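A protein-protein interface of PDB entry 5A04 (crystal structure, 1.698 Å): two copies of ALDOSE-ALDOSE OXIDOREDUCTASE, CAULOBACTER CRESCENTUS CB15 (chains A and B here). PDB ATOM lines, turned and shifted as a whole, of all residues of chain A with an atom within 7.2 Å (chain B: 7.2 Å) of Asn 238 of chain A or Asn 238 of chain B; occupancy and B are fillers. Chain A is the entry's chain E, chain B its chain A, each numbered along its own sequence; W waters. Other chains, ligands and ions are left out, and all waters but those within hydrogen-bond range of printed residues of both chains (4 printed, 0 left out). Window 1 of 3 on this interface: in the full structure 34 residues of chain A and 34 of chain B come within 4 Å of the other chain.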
ATOM      1  N   THR A 156      31.905  -6.983  13.059  1.00  0.00           N
ATOM      2  CA  THR A 156      30.890  -5.930  13.093  1.00  0.00           C
ATOM      3  C   THR A 156      29.487  -6.495  13.166  1.00  0.00           C
ATOM      4  O   THR A 156      29.189  -7.529  12.565  1.00  0.00           O
ATOM      5  CB  THR A 156      30.953  -5.004  11.849  1.00  0.00           C
ATOM      6  OG1 THR A 156      30.682  -5.771  10.666  1.00  0.00           O
ATOM      7  CG2 THR A 156      32.323  -4.319  11.719  1.00  0.00           C
ATOM      8  N   VAL A 157      28.628  -5.804  13.911  1.00  0.00           N
ATOM      9  CA  VAL A 157      27.186  -6.017  13.858  1.00  0.00           C
ATOM     10  C   VAL A 157      26.566  -4.668  13.542  1.00  0.00           C
ATOM     11  O   VAL A 157      26.810  -3.689  14.244  1.00  0.00           O
ATOM     12  CB  VAL A 157      26.601  -6.562  15.179  1.00  0.00           C
ATOM     13  CG1 VAL A 157      25.081  -6.617  15.093  1.00  0.00           C
ATOM     14  CG2 VAL A 157      27.185  -7.944  15.491  1.00  0.00           C
ATOM     15  N   VAL A 158      25.813  -4.599  12.454  1.00  0.00           N
ATOM     16  CA  VAL A 158      25.121  -3.370  12.087  1.00  0.00           C
ATOM     17  C   VAL A 158      23.636  -3.670  12.105  1.00  0.00           C
ATOM     18  O   VAL A 158      23.161  -4.494  11.335  1.00  0.00           O
ATOM     19  CB  VAL A 158      25.568  -2.850  10.702  1.00  0.00           C
ATOM     20  CG1 VAL A 158      24.767  -1.609  10.273  1.00  0.00           C
ATOM     21  CG2 VAL A 158      27.056  -2.542  10.731  1.00  0.00           C
ATOM     22  N   THR A 159      22.905  -3.013  12.997  1.00  0.00           N
ATOM     23  CA  THR A 159      21.513  -3.371  13.211  1.00  0.00           C
ATOM     24  C   THR A 159      20.668  -2.127  13.454  1.00  0.00           C
ATOM     25  O   THR A 159      21.051  -1.235  14.222  1.00  0.00           O
ATOM     26  CB  THR A 159      21.382  -4.375  14.380  1.00  0.00           C
ATOM     27  OG1 THR A 159      20.006  -4.682  14.632  1.00  0.00           O
ATOM     28  CG2 THR A 159      22.040  -3.825  15.657  1.00  0.00           C
ATOM     29  N   ASP A 160      19.524  -2.064  12.773  1.00  0.00           N
ATOM     30  CA  ASP A 160      18.639  -0.907  12.838  1.00  0.00           C
ATOM     31  C   ASP A 160      17.230  -1.370  13.185  1.00  0.00           C
ATOM     32  O   ASP A 160      16.676  -2.234  12.505  1.00  0.00           O
ATOM     33  CB  ASP A 160      18.579  -0.136  11.504  1.00  0.00           C
ATOM     34  CG  ASP A 160      19.950   0.182  10.916  1.00  0.00           C
ATOM     35  OD1 ASP A 160      20.924   0.404  11.677  1.00  0.00           O
ATOM     36  OD2 ASP A 160      20.041   0.243   9.664  1.00  0.00           O
ATOM     37  N   SER A 190      17.868  -4.017  18.709  1.00  0.00           N
ATOM     38  CA  SER A 190      19.214  -3.842  18.164  1.00  0.00           C
ATOM     39  C   SER A 190      20.253  -4.242  19.195  1.00  0.00           C
ATOM     40  O   SER A 190      21.218  -4.941  18.898  1.00  0.00           O
ATOM     41  CB  SER A 190      19.456  -2.390  17.738  1.00  0.00           C
ATOM     42  OG  SER A 190      18.610  -1.988  16.667  1.00  0.00           O
ATOM     43  N   ALA A 194      22.762  -7.467  19.107  1.00  0.00           N
ATOM     44  CA  ALA A 194      24.215  -7.297  19.166  1.00  0.00           C
ATOM     45  C   ALA A 194      24.814  -8.233  20.226  1.00  0.00           C
ATOM     46  O   ALA A 194      25.874  -8.830  20.028  1.00  0.00           O
ATOM     47  CB  ALA A 194      24.581  -5.843  19.461  1.00  0.00           C
ATOM     48  N   VAL A 208      24.392   8.927  20.269  1.00  0.00           N
ATOM     49  CA  VAL A 208      23.943  10.209  19.742  1.00  0.00           C
ATOM     50  C   VAL A 208      22.421  10.202  19.766  1.00  0.00           C
ATOM     51  O   VAL A 208      21.808   9.256  19.274  1.00  0.00           O
ATOM     52  CB  VAL A 208      24.406  10.436  18.274  1.00  0.00           C
ATOM     53  CG1 VAL A 208      23.722  11.660  17.689  1.00  0.00           C
ATOM     54  CG2 VAL A 208      25.933  10.558  18.180  1.00  0.00           C
ATOM     55  N   ILE A 225      17.912   7.472  19.003  1.00  0.00           N
ATOM     56  CA  ILE A 225      19.147   7.405  19.763  1.00  0.00           C
ATOM     57  C   ILE A 225      19.965   6.252  19.188  1.00  0.00           C
ATOM     58  O   ILE A 225      19.594   5.079  19.298  1.00  0.00           O
ATOM     59  CB  ILE A 225      18.891   7.265  21.296  1.00  0.00           C
ATOM     60  CG1 ILE A 225      20.221   7.234  22.063  1.00  0.00           C
ATOM     61  CG2 ILE A 225      17.967   6.077  21.628  1.00  0.00           C
ATOM     62  CD1 ILE A 225      20.081   7.552  23.554  1.00  0.00           C
ATOM     63  N   ASN A 226      21.044   6.606  18.498  1.00  0.00           N
ATOM     64  CA  ASN A 226      21.888   5.617  17.846  1.00  0.00           C
ATOM     65  C   ASN A 226      23.090   5.355  18.726  1.00  0.00           C
ATOM     66  O   ASN A 226      23.556   6.256  19.417  1.00  0.00           O
ATOM     67  CB  ASN A 226      22.316   6.093  16.461  1.00  0.00           C
ATOM     68  CG  ASN A 226      21.142   6.341  15.550  1.00  0.00           C
ATOM     69  OD1 ASN A 226      20.083   5.725  15.705  1.00  0.00           O
ATOM     70  ND2 ASN A 226      21.315   7.249  14.591  1.00  0.00           N
ATOM     71  N   PHE A 227      23.587   4.127  18.742  1.00  0.00           N
ATOM     72  CA  PHE A 227      24.669   3.840  19.674  1.00  0.00           C
ATOM     73  C   PHE A 227      25.695   2.891  19.096  1.00  0.00           C
ATOM     74  O   PHE A 227      25.419   2.146  18.145  1.00  0.00           O
ATOM     75  CB  PHE A 227      24.127   3.277  21.006  1.00  0.00           C
ATOM     76  CG  PHE A 227      23.141   2.136  20.862  1.00  0.00           C
ATOM     77  CD1 PHE A 227      21.797   2.389  20.600  1.00  0.00           C
ATOM     78  CD2 PHE A 227      23.544   0.821  21.084  1.00  0.00           C
ATOM     79  CE1 PHE A 227      20.882   1.349  20.511  1.00  0.00           C
ATOM     80  CE2 PHE A 227      22.635  -0.225  20.997  1.00  0.00           C
ATOM     81  CZ  PHE A 227      21.295   0.047  20.705  1.00  0.00           C
ATOM     82  N   GLN A 228      26.894   2.963  19.664  1.00  0.00           N
ATOM     83  CA  GLN A 228      27.994   2.081  19.301  1.00  0.00           C
ATOM     84  C   GLN A 228      28.388   1.232  20.490  1.00  0.00           C
ATOM     85  O   GLN A 228      28.436   1.731  21.612  1.00  0.00           O
ATOM     86  CB  GLN A 228      29.220   2.876  18.848  1.00  0.00           C
ATOM     87  CG  GLN A 228      28.920   3.988  17.858  1.00  0.00           C
ATOM     88  CD  GLN A 228      30.210   4.600  17.343  1.00  0.00           C
ATOM     89  OE1 GLN A 228      30.857   5.369  18.047  1.00  0.00           O
ATOM     90  NE2 GLN A 228      30.620   4.212  16.123  1.00  0.00           N
ATOM     91  N   LEU A 229      28.704  -0.032  20.228  1.00  0.00           N
ATOM     92  CA  LEU A 229      29.170  -0.948  21.261  1.00  0.00           C
ATOM     93  C   LEU A 229      30.522  -1.542  20.909  1.00  0.00           C
ATOM     94  O   LEU A 229      30.750  -1.941  19.769  1.00  0.00           O
ATOM     95  CB  LEU A 229      28.155  -2.085  21.469  1.00  0.00           C
ATOM     96  CG  LEU A 229      26.707  -1.676  21.711  1.00  0.00           C
ATOM     97  CD1 LEU A 229      25.797  -2.914  21.656  1.00  0.00           C
ATOM     98  CD2 LEU A 229      26.576  -0.978  23.062  1.00  0.00           C
ATOM     99  N   THR A 236      32.547  -5.128  17.257  1.00  0.00           N
ATOM    100  CA  THR A 236      31.899  -3.821  17.363  1.00  0.00           C
ATOM    101  C   THR A 236      30.464  -3.903  16.883  1.00  0.00           C
ATOM    102  O   THR A 236      30.119  -4.774  16.085  1.00  0.00           O
ATOM    103  CB  THR A 236      32.627  -2.731  16.517  1.00  0.00           C
ATOM    104  OG1 THR A 236      32.575  -3.094  15.124  1.00  0.00           O
ATOM    105  CG2 THR A 236      34.076  -2.571  16.956  1.00  0.00           C
ATOM    106  N   ALA A 237      29.633  -2.973  17.338  1.00  0.00           N
ATOM    107  CA  ALA A 237      28.271  -2.866  16.837  1.00  0.00           C
ATOM    108  C   ALA A 237      27.892  -1.411  16.597  1.00  0.00           C
ATOM    109  O   ALA A 237      28.209  -0.540  17.408  1.00  0.00           O
ATOM    110  CB  ALA A 237      27.280  -3.523  17.816  1.00  0.00           C
ATOM    111  N   ASN A 238      27.237  -1.150  15.466  1.00  0.00           N
ATOM    112  CA  ASN A 238      26.614   0.144  15.194  1.00  0.00           C
ATOM    113  C   ASN A 238      25.126  -0.090  15.187  1.00  0.00           C
ATOM    114  O   ASN A 238      24.645  -0.899  14.381  1.00  0.00           O
ATOM    115  CB  ASN A 238      27.015   0.715  13.822  1.00  0.00           C
ATOM    116  CG  ASN A 238      28.217   1.642  13.864  1.00  0.00           C
ATOM    117  OD1 ASN A 238      28.820   1.901  14.911  1.00  0.00           O
ATOM    118  ND2 ASN A 238      28.575   2.151  12.690  1.00  0.00           N
ATOM    119  N   CYS A 239      24.392   0.614  16.036  1.00  0.00           N
ATOM    120  CA  CYS A 239      22.959   0.345  16.192  1.00  0.00           C
ATOM    121  C   CYS A 239      22.099   1.587  16.010  1.00  0.00           C
ATOM    122  O   CYS A 239      22.448   2.664  16.498  1.00  0.00           O
ATOM    123  CB  CYS A 239      22.683  -0.232  17.580  1.00  0.00           C
ATOM    124  SG  CYS A 239      23.720  -1.620  18.030  1.00  0.00           S
ATOM    125  N   VAL A 240      20.966   1.426  15.324  1.00  0.00           N
ATOM    126  CA  VAL A 240      19.946   2.471  15.255  1.00  0.00           C
ATOM    127  C   VAL A 240      18.710   2.094  16.078  1.00  0.00           C
ATOM    128  O   VAL A 240      18.285   0.936  16.082  1.00  0.00           O
ATOM    129  CB  VAL A 240      19.526   2.750  13.792  1.00  0.00           C
ATOM    130  CG1 VAL A 240      18.228   3.567  13.722  1.00  0.00           C
ATOM    131  CG2 VAL A 240      20.650   3.460  13.063  1.00  0.00           C
ATOM    132  N   SER A 241      18.183   3.084  16.804  1.00  0.00           N
ATOM    133  CA  SER A 241      16.902   3.019  17.502  1.00  0.00           C
ATOM    134  C   SER A 241      16.091   4.241  17.079  1.00  0.00           C
ATOM    135  O   SER A 241      16.565   5.373  17.234  1.00  0.00           O
ATOM    136  CB  SER A 241      17.108   3.020  19.024  1.00  0.00           C
ATOM    137  OG  SER A 241      15.870   3.012  19.710  1.00  0.00           O
ATOM    138  N   ARG A 251      22.973  -7.102  10.146  1.00  0.00           N
ATOM    139  CA  ARG A 251      23.989  -7.886   9.470  1.00  0.00           C
ATOM    140  C   ARG A 251      25.129  -8.121  10.430  1.00  0.00           C
ATOM    141  O   ARG A 251      25.593  -7.184  11.087  1.00  0.00           O
ATOM    142  CB  ARG A 251      24.503  -7.188   8.203  1.00  0.00           C
ATOM    143  CG  ARG A 251      25.643  -7.976   7.549  1.00  0.00           C
ATOM    144  CD  ARG A 251      26.289  -7.248   6.369  1.00  0.00           C
ATOM    145  NE  ARG A 251      25.339  -6.973   5.285  1.00  0.00           N
ATOM    146  CZ  ARG A 251      25.676  -6.391   4.137  1.00  0.00           C
ATOM    147  NH1 ARG A 251      26.941  -6.021   3.923  1.00  0.00           N
ATOM    148  NH2 ARG A 251      24.747  -6.167   3.204  1.00  0.00           N
ATOM    149  N   THR B 156      18.139   9.147   9.179  1.00  0.00           N
ATOM    150  CA  THR B 156      19.298   8.273   9.371  1.00  0.00           C
ATOM    151  C   THR B 156      20.016   7.941   8.066  1.00  0.00           C
ATOM    152  O   THR B 156      19.394   7.792   7.011  1.00  0.00           O
ATOM    153  CB  THR B 156      18.919   6.927  10.055  1.00  0.00           C
ATOM    154  OG1 THR B 156      18.017   6.190   9.215  1.00  0.00           O
ATOM    155  CG2 THR B 156      18.258   7.154  11.413  1.00  0.00           C
ATOM    156  N   VAL B 157      21.335   7.847   8.153  1.00  0.00           N
ATOM    157  CA  VAL B 157      22.155   7.268   7.103  1.00  0.00           C
ATOM    158  C   VAL B 157      22.950   6.158   7.754  1.00  0.00           C
ATOM    159  O   VAL B 157      23.682   6.406   8.721  1.00  0.00           O
ATOM    160  CB  VAL B 157      23.128   8.271   6.468  1.00  0.00           C
ATOM    161  CG1 VAL B 157      23.978   7.562   5.416  1.00  0.00           C
ATOM    162  CG2 VAL B 157      22.369   9.427   5.835  1.00  0.00           C
ATOM    163  N   VAL B 158      22.800   4.934   7.263  1.00  0.00           N
ATOM    164  CA  VAL B 158      23.586   3.829   7.792  1.00  0.00           C
ATOM    165  C   VAL B 158      24.440   3.297   6.653  1.00  0.00           C
ATOM    166  O   VAL B 158      23.908   2.791   5.658  1.00  0.00           O
ATOM    167  CB  VAL B 158      22.692   2.707   8.387  1.00  0.00           C
ATOM    168  CG1 VAL B 158      23.525   1.490   8.784  1.00  0.00           C
ATOM    169  CG2 VAL B 158      21.907   3.231   9.603  1.00  0.00           C
ATOM    170  N   THR B 159      25.756   3.433   6.782  1.00  0.00           N
ATOM    171  CA  THR B 159      26.639   3.120   5.665  1.00  0.00           C
ATOM    172  C   THR B 159      27.898   2.406   6.146  1.00  0.00           C
ATOM    173  O   THR B 159      28.534   2.803   7.137  1.00  0.00           O
ATOM    174  CB  THR B 159      26.989   4.410   4.847  1.00  0.00           C
ATOM    175  OG1 THR B 159      27.908   4.091   3.794  1.00  0.00           O
ATOM    176  CG2 THR B 159      27.609   5.516   5.740  1.00  0.00           C
ATOM    177  N   ASP B 160      28.225   1.318   5.451  1.00  0.00           N
ATOM    178  CA  ASP B 160      29.330   0.440   5.811  1.00  0.00           C
ATOM    179  C   ASP B 160      30.272   0.297   4.626  1.00  0.00           C
ATOM    180  O   ASP B 160      29.828  -0.050   3.531  1.00  0.00           O
ATOM    181  CB  ASP B 160      28.827  -0.958   6.198  1.00  0.00           C
ATOM    182  CG  ASP B 160      27.766  -0.935   7.274  1.00  0.00           C
ATOM    183  OD1 ASP B 160      27.775  -0.014   8.121  1.00  0.00           O
ATOM    184  OD2 ASP B 160      26.919  -1.861   7.276  1.00  0.00           O
ATOM    185  N   SER B 190      32.147   6.015   3.366  1.00  0.00           N
ATOM    186  CA  SER B 190      31.009   6.138   4.283  1.00  0.00           C
ATOM    187  C   SER B 190      30.791   7.598   4.670  1.00  0.00           C
ATOM    188  O   SER B 190      29.665   8.089   4.706  1.00  0.00           O
ATOM    189  CB  SER B 190      31.236   5.303   5.552  1.00  0.00           C
ATOM    190  OG  SER B 190      31.314   3.922   5.253  1.00  0.00           O
ATOM    191  N   ALA B 194      27.676  10.033   3.604  1.00  0.00           N
ATOM    192  CA  ALA B 194      26.820  10.654   4.618  1.00  0.00           C
ATOM    193  C   ALA B 194      26.669  12.143   4.314  1.00  0.00           C
ATOM    194  O   ALA B 194      25.577  12.705   4.431  1.00  0.00           O
ATOM    195  CB  ALA B 194      27.387  10.443   6.015  1.00  0.00           C
ATOM    196  N   VAL B 208      34.514   4.676  17.651  1.00  0.00           N
ATOM    197  CA  VAL B 208      35.121   3.564  18.374  1.00  0.00           C
ATOM    198  C   VAL B 208      36.109   2.872  17.437  1.00  0.00           C
ATOM    199  O   VAL B 208      35.771   2.583  16.281  1.00  0.00           O
ATOM    200  CB  VAL B 208      34.054   2.550  18.877  1.00  0.00           C
ATOM    201  CG1 VAL B 208      33.173   3.184  19.938  1.00  0.00           C
ATOM    202  CG2 VAL B 208      33.200   2.063  17.751  1.00  0.00           C
ATOM    203  N   ILE B 225      37.336   1.378  12.451  1.00  0.00           N
ATOM    204  CA  ILE B 225      36.982   2.587  13.192  1.00  0.00           C
ATOM    205  C   ILE B 225      35.597   3.037  12.724  1.00  0.00           C
ATOM    206  O   ILE B 225      35.403   3.543  11.616  1.00  0.00           O
ATOM    207  CB  ILE B 225      38.067   3.711  13.067  1.00  0.00           C
ATOM    208  CG1 ILE B 225      37.674   4.923  13.921  1.00  0.00           C
ATOM    209  CG2 ILE B 225      38.352   4.105  11.595  1.00  0.00           C
ATOM    210  CD1 ILE B 225      38.822   5.939  14.087  1.00  0.00           C
ATOM    211  N   ASN B 226      34.614   2.780  13.581  1.00  0.00           N
ATOM    212  CA  ASN B 226      33.226   3.091  13.275  1.00  0.00           C
ATOM    213  C   ASN B 226      32.895   4.431  13.875  1.00  0.00           C
ATOM    214  O   ASN B 226      33.417   4.779  14.941  1.00  0.00           O
ATOM    215  CB  ASN B 226      32.295   2.005  13.823  1.00  0.00           C
ATOM    216  CG  ASN B 226      32.612   0.639  13.248  1.00  0.00           C
ATOM    217  OD1 ASN B 226      33.168   0.529  12.142  1.00  0.00           O
ATOM    218  ND2 ASN B 226      32.260  -0.412  13.988  1.00  0.00           N
ATOM    219  N   PHE B 227      32.046   5.197  13.212  1.00  0.00           N
ATOM    220  CA  PHE B 227      31.785   6.540  13.702  1.00  0.00           C
ATOM    221  C   PHE B 227      30.338   6.945  13.530  1.00  0.00           C
ATOM    222  O   PHE B 227      29.591   6.377  12.717  1.00  0.00           O
ATOM    223  CB  PHE B 227      32.727   7.565  13.033  1.00  0.00           C
ATOM    224  CG  PHE B 227      32.779   7.490  11.523  1.00  0.00           C
ATOM    225  CD1 PHE B 227      33.583   6.547  10.878  1.00  0.00           C
ATOM    226  CD2 PHE B 227      32.066   8.403  10.751  1.00  0.00           C
ATOM    227  CE1 PHE B 227      33.639   6.497   9.464  1.00  0.00           C
ATOM    228  CE2 PHE B 227      32.132   8.364   9.351  1.00  0.00           C
ATOM    229  CZ  PHE B 227      32.914   7.411   8.714  1.00  0.00           C
ATOM    230  N   GLN B 228      29.929   7.895  14.368  1.00  0.00           N
ATOM    231  CA  GLN B 228      28.590   8.459  14.322  1.00  0.00           C
ATOM    232  C   GLN B 228      28.715   9.927  13.977  1.00  0.00           C
ATOM    233  O   GLN B 228      29.623  10.590  14.475  1.00  0.00           O
ATOM    234  CB  GLN B 228      27.886   8.331  15.671  1.00  0.00           C
ATOM    235  CG  GLN B 228      27.822   6.921  16.207  1.00  0.00           C
ATOM    236  CD  GLN B 228      26.970   6.850  17.446  1.00  0.00           C
ATOM    237  OE1 GLN B 228      27.350   7.372  18.503  1.00  0.00           O
ATOM    238  NE2 GLN B 228      25.794   6.216  17.330  1.00  0.00           N
ATOM    239  N   LEU B 229      27.802  10.423  13.147  1.00  0.00           N
ATOM    240  CA  LEU B 229      27.745  11.841  12.808  1.00  0.00           C
ATOM    241  C   LEU B 229      26.381  12.411  13.143  1.00  0.00           C
ATOM    242  O   LEU B 229      25.354  11.771  12.899  1.00  0.00           O
ATOM    243  CB  LEU B 229      28.027  12.060  11.312  1.00  0.00           C
ATOM    244  CG  LEU B 229      29.303  11.442  10.734  1.00  0.00           C
ATOM    245  CD1 LEU B 229      29.330  11.590   9.217  1.00  0.00           C
ATOM    246  CD2 LEU B 229      30.538  12.076  11.349  1.00  0.00           C
ATOM    247  N   THR B 236      21.163  11.960  11.341  1.00  0.00           N
ATOM    248  CA  THR B 236      22.218  11.188  11.993  1.00  0.00           C
ATOM    249  C   THR B 236      22.841  10.202  11.011  1.00  0.00           C
ATOM    250  O   THR B 236      22.196   9.790  10.045  1.00  0.00           O
ATOM    251  CB  THR B 236      21.677  10.398  13.209  1.00  0.00           C
ATOM    252  OG1 THR B 236      20.723   9.425  12.751  1.00  0.00           O
ATOM    253  CG2 THR B 236      20.987  11.340  14.195  1.00  0.00           C
ATOM    254  N   ALA B 237      24.090   9.813  11.249  1.00  0.00           N
ATOM    255  CA  ALA B 237      24.679   8.728  10.467  1.00  0.00           C
ATOM    256  C   ALA B 237      25.461   7.780  11.365  1.00  0.00           C
ATOM    257  O   ALA B 237      26.156   8.205  12.293  1.00  0.00           O
ATOM    258  CB  ALA B 237      25.582   9.271   9.346  1.00  0.00           C
ATOM    259  N   ASN B 238      25.296   6.486  11.101  1.00  0.00           N
ATOM    260  CA  ASN B 238      26.104   5.416  11.694  1.00  0.00           C
ATOM    261  C   ASN B 238      26.965   4.842  10.592  1.00  0.00           C
ATOM    262  O   ASN B 238      26.414   4.337   9.602  1.00  0.00           O
ATOM    263  CB  ASN B 238      25.243   4.274  12.244  1.00  0.00           C
ATOM    264  CG  ASN B 238      24.906   4.410  13.711  1.00  0.00           C
ATOM    265  OD1 ASN B 238      25.276   5.381  14.378  1.00  0.00           O
ATOM    266  ND2 ASN B 238      24.171   3.422  14.219  1.00  0.00           N
ATOM    267  N   CYS B 239      28.282   4.874  10.773  1.00  0.00           N
ATOM    268  CA  CYS B 239      29.220   4.513   9.715  1.00  0.00           C
ATOM    269  C   CYS B 239      30.210   3.444  10.147  1.00  0.00           C
ATOM    270  O   CYS B 239      30.796   3.524  11.236  1.00  0.00           O
ATOM    271  CB  CYS B 239      29.987   5.760   9.264  1.00  0.00           C
ATOM    272  SG  CYS B 239      28.937   7.151   8.726  1.00  0.00           S
ATOM    273  N   VAL B 240      30.427   2.459   9.279  1.00  0.00           N
ATOM    274  CA  VAL B 240      31.490   1.481   9.486  1.00  0.00           C
ATOM    275  C   VAL B 240      32.656   1.730   8.528  1.00  0.00           C
ATOM    276  O   VAL B 240      32.440   1.999   7.347  1.00  0.00           O
ATOM    277  CB  VAL B 240      30.968   0.034   9.296  1.00  0.00           C
ATOM    278  CG1 VAL B 240      32.123  -0.949   9.072  1.00  0.00           C
ATOM    279  CG2 VAL B 240      30.110  -0.382  10.500  1.00  0.00           C
ATOM    280  N   SER B 241      33.879   1.641   9.057  1.00  0.00           N
ATOM    281  CA  SER B 241      35.115   1.626   8.268  1.00  0.00           C
ATOM    282  C   SER B 241      35.938   0.431   8.726  1.00  0.00           C
ATOM    283  O   SER B 241      36.225   0.318   9.923  1.00  0.00           O
ATOM    284  CB  SER B 241      35.912   2.925   8.478  1.00  0.00           C
ATOM    285  OG  SER B 241      37.134   2.884   7.762  1.00  0.00           O
ATOM    286  N   ARG B 251      22.103   2.937   3.369  1.00  0.00           N
ATOM    287  CA  ARG B 251      20.668   3.180   3.353  1.00  0.00           C
ATOM    288  C   ARG B 251      20.413   4.548   3.966  1.00  0.00           C
ATOM    289  O   ARG B 251      20.934   4.849   5.047  1.00  0.00           O
ATOM    290  CB  ARG B 251      19.889   2.110   4.128  1.00  0.00           C
ATOM    291  CG  ARG B 251      18.386   2.402   4.104  1.00  0.00           C
ATOM    292  CD  ARG B 251      17.578   1.471   4.979  1.00  0.00           C
ATOM    293  NE  ARG B 251      17.632   0.090   4.512  1.00  0.00           N
ATOM    294  CZ  ARG B 251      16.902  -0.893   5.027  1.00  0.00           C
ATOM    295  NH1 ARG B 251      16.069  -0.652   6.038  1.00  0.00           N
ATOM    296  NH2 ARG B 251      17.011  -2.119   4.540  1.00  0.00           N
HETATM  297  O   HOH W   1      23.391   1.094  12.590  1.00  0.00           O
HETATM  298  O   HOH W   2      30.703   0.521  16.451  1.00  0.00           O
HETATM  299  O   HOH W   3      27.027   1.499  10.234  1.00  0.00           O
HETATM  300  O   HOH W   4      24.291   8.089  14.512  1.00  0.00           O
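Water W2 lies within hydrogen-bond range of the side-chain amide oxygen (OD1) of Asn 238 of chain A (2.8 Å), the backbone carbonyl oxygen (O) of Ala 237 of chain A (2.9 Å) and the side-chain amide nitrogen (ND2) of Asn 226 of chain B (3.1 Å).
Of the printed residues of chain B, Gln 228 of chain A touches Val 208 (3.7 Å), Asn 226 (3.1 Å), Phe 227 (3.4 Å) and Gln 228 (3.5 Å).
Of chain B, only Asn 226 (3.6 Å), Asn 238 (3.8 Å), Cys 239 (3.0 Å) and Val 240 (3.7 Å) come within 4 Å of Asn 238 of chain A.
Printed residues of chain B within 4 Å of Cys 239 of chain A: Asn 238 (3.0 Å).
Of the printed residues of chain A, Asp 160 of chain B touches Val 158 (3.5 Å).
Leu 229 of chain B touches none of the printed residues of chain A.
Asn 238 of chain B touches just these residues of chain A: Asn 226 (3.7 Å), Asn 238 (3.8 Å), Cys 239 (3.0 Å) and Val 240 (3.7 Å).
The nearest printed residue of chain A that does not touch Val 158 of chain B is Asn 238 of chain A (6.2 Å).
Printed residues of chain A that touch a printed residue of chain B: Val 158, Asp 160, Val 208, Asn 226, Phe 227, Gln 228, Thr 236, Asn 238, Cys 239 and Val 240.
Along chain A the printed residues that touch a printed residue of chain B span positions 158 to 240.
Among the printed residues, 21 pairs touch across the chains.
Among the printed residues, no Asp or Glu carboxylate lies within 4 Å of a Lys or Arg side-chain nitrogen of the other chain.
The backbone carbonyl oxygen (O) of Thr 159 of chain B sits at hydrogen-bond distance from the backbone NH (N) of Val 240 of chain B, at 2.9 Å.
The backbone NH (N) of Val 208 of chain B is in hydrogen-bond range of the backbone carbonyl oxygen (O) of Asn 226 of chain B (2.9 Å).
O of Asn 238 of chain A lies within hydrogen-bond range of N of Thr 159 of chain A (3.1 Å).
Among the printed residues, merely in contact across the chains: Gln 228 of chain A with Gln 228 of chain B, Val 208 of chain A with Gln 228 of chain B, Asp 160 of chain A with Val 158 of chain B, Val 158 of chain A with Asp 160 of chain B, Asn 238 of chain A with Asn 226 of chain B, Val 158 of chain A with Val 158 of chain B, Asn 238 of chain A with Val 240 of chain B, Val 240 of chain A with Val 158 of chain B, Asn 226 of chain A with Asn 238 of chain B, Gln 228 of chain A with Val 208 of chain B, Val 240 of chain A with Asn 238 of chain B, Val 158 of chain A with Val 240 of chain B and Asn 238 of chain A with Asn 238 of chain B.
O of Asn 226 of chain B sits at hydrogen-bond distance from NE2 of Gln 228 of chain A (3.1 Å).
The side-chain hydroxyl (OG1) of Thr 236 of chain A lies within hydrogen-bond range of the side-chain amide nitrogen (ND2) of Asn 226 of chain B, at 2.9 Å.
The backbone NH of Phe 227 of chain B sits close to the side-chain amide nitrogen of Gln 228 of chain A, at 3.4 Å.
NE2 of Gln 228 of chain B lies within hydrogen-bond range of O of Asn 226 of chain A (3.1 Å).
NE2 of Gln 228 of chain B sits close to N of Phe 227 of chain A, 3.4 Å away.
OG1 of Thr 236 of chain B is in hydrogen-bond range of ND2 of Asn 226 of chain A.
The backbone carbonyl oxygen of Cys 239 of chain A sits at hydrogen-bond distance from the side-chain amide nitrogen of Asn 238 of chain B.
The side-chain amide nitrogen (ND2) of Asn 238 of chain A lies within hydrogen-bond range of the backbone carbonyl oxygen (O) of Cys 239 of chain B, at 3.0 Å.
Gln 228 of chain B touches its own counterpart, Gln 228 of chain A.
Asn 238 of chain B touches its own counterpart, Asn 238 of chain A.
Of the 21 pairs that touch across the chains among the printed residues, 21 have their exchanged pair printed and touching as well.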
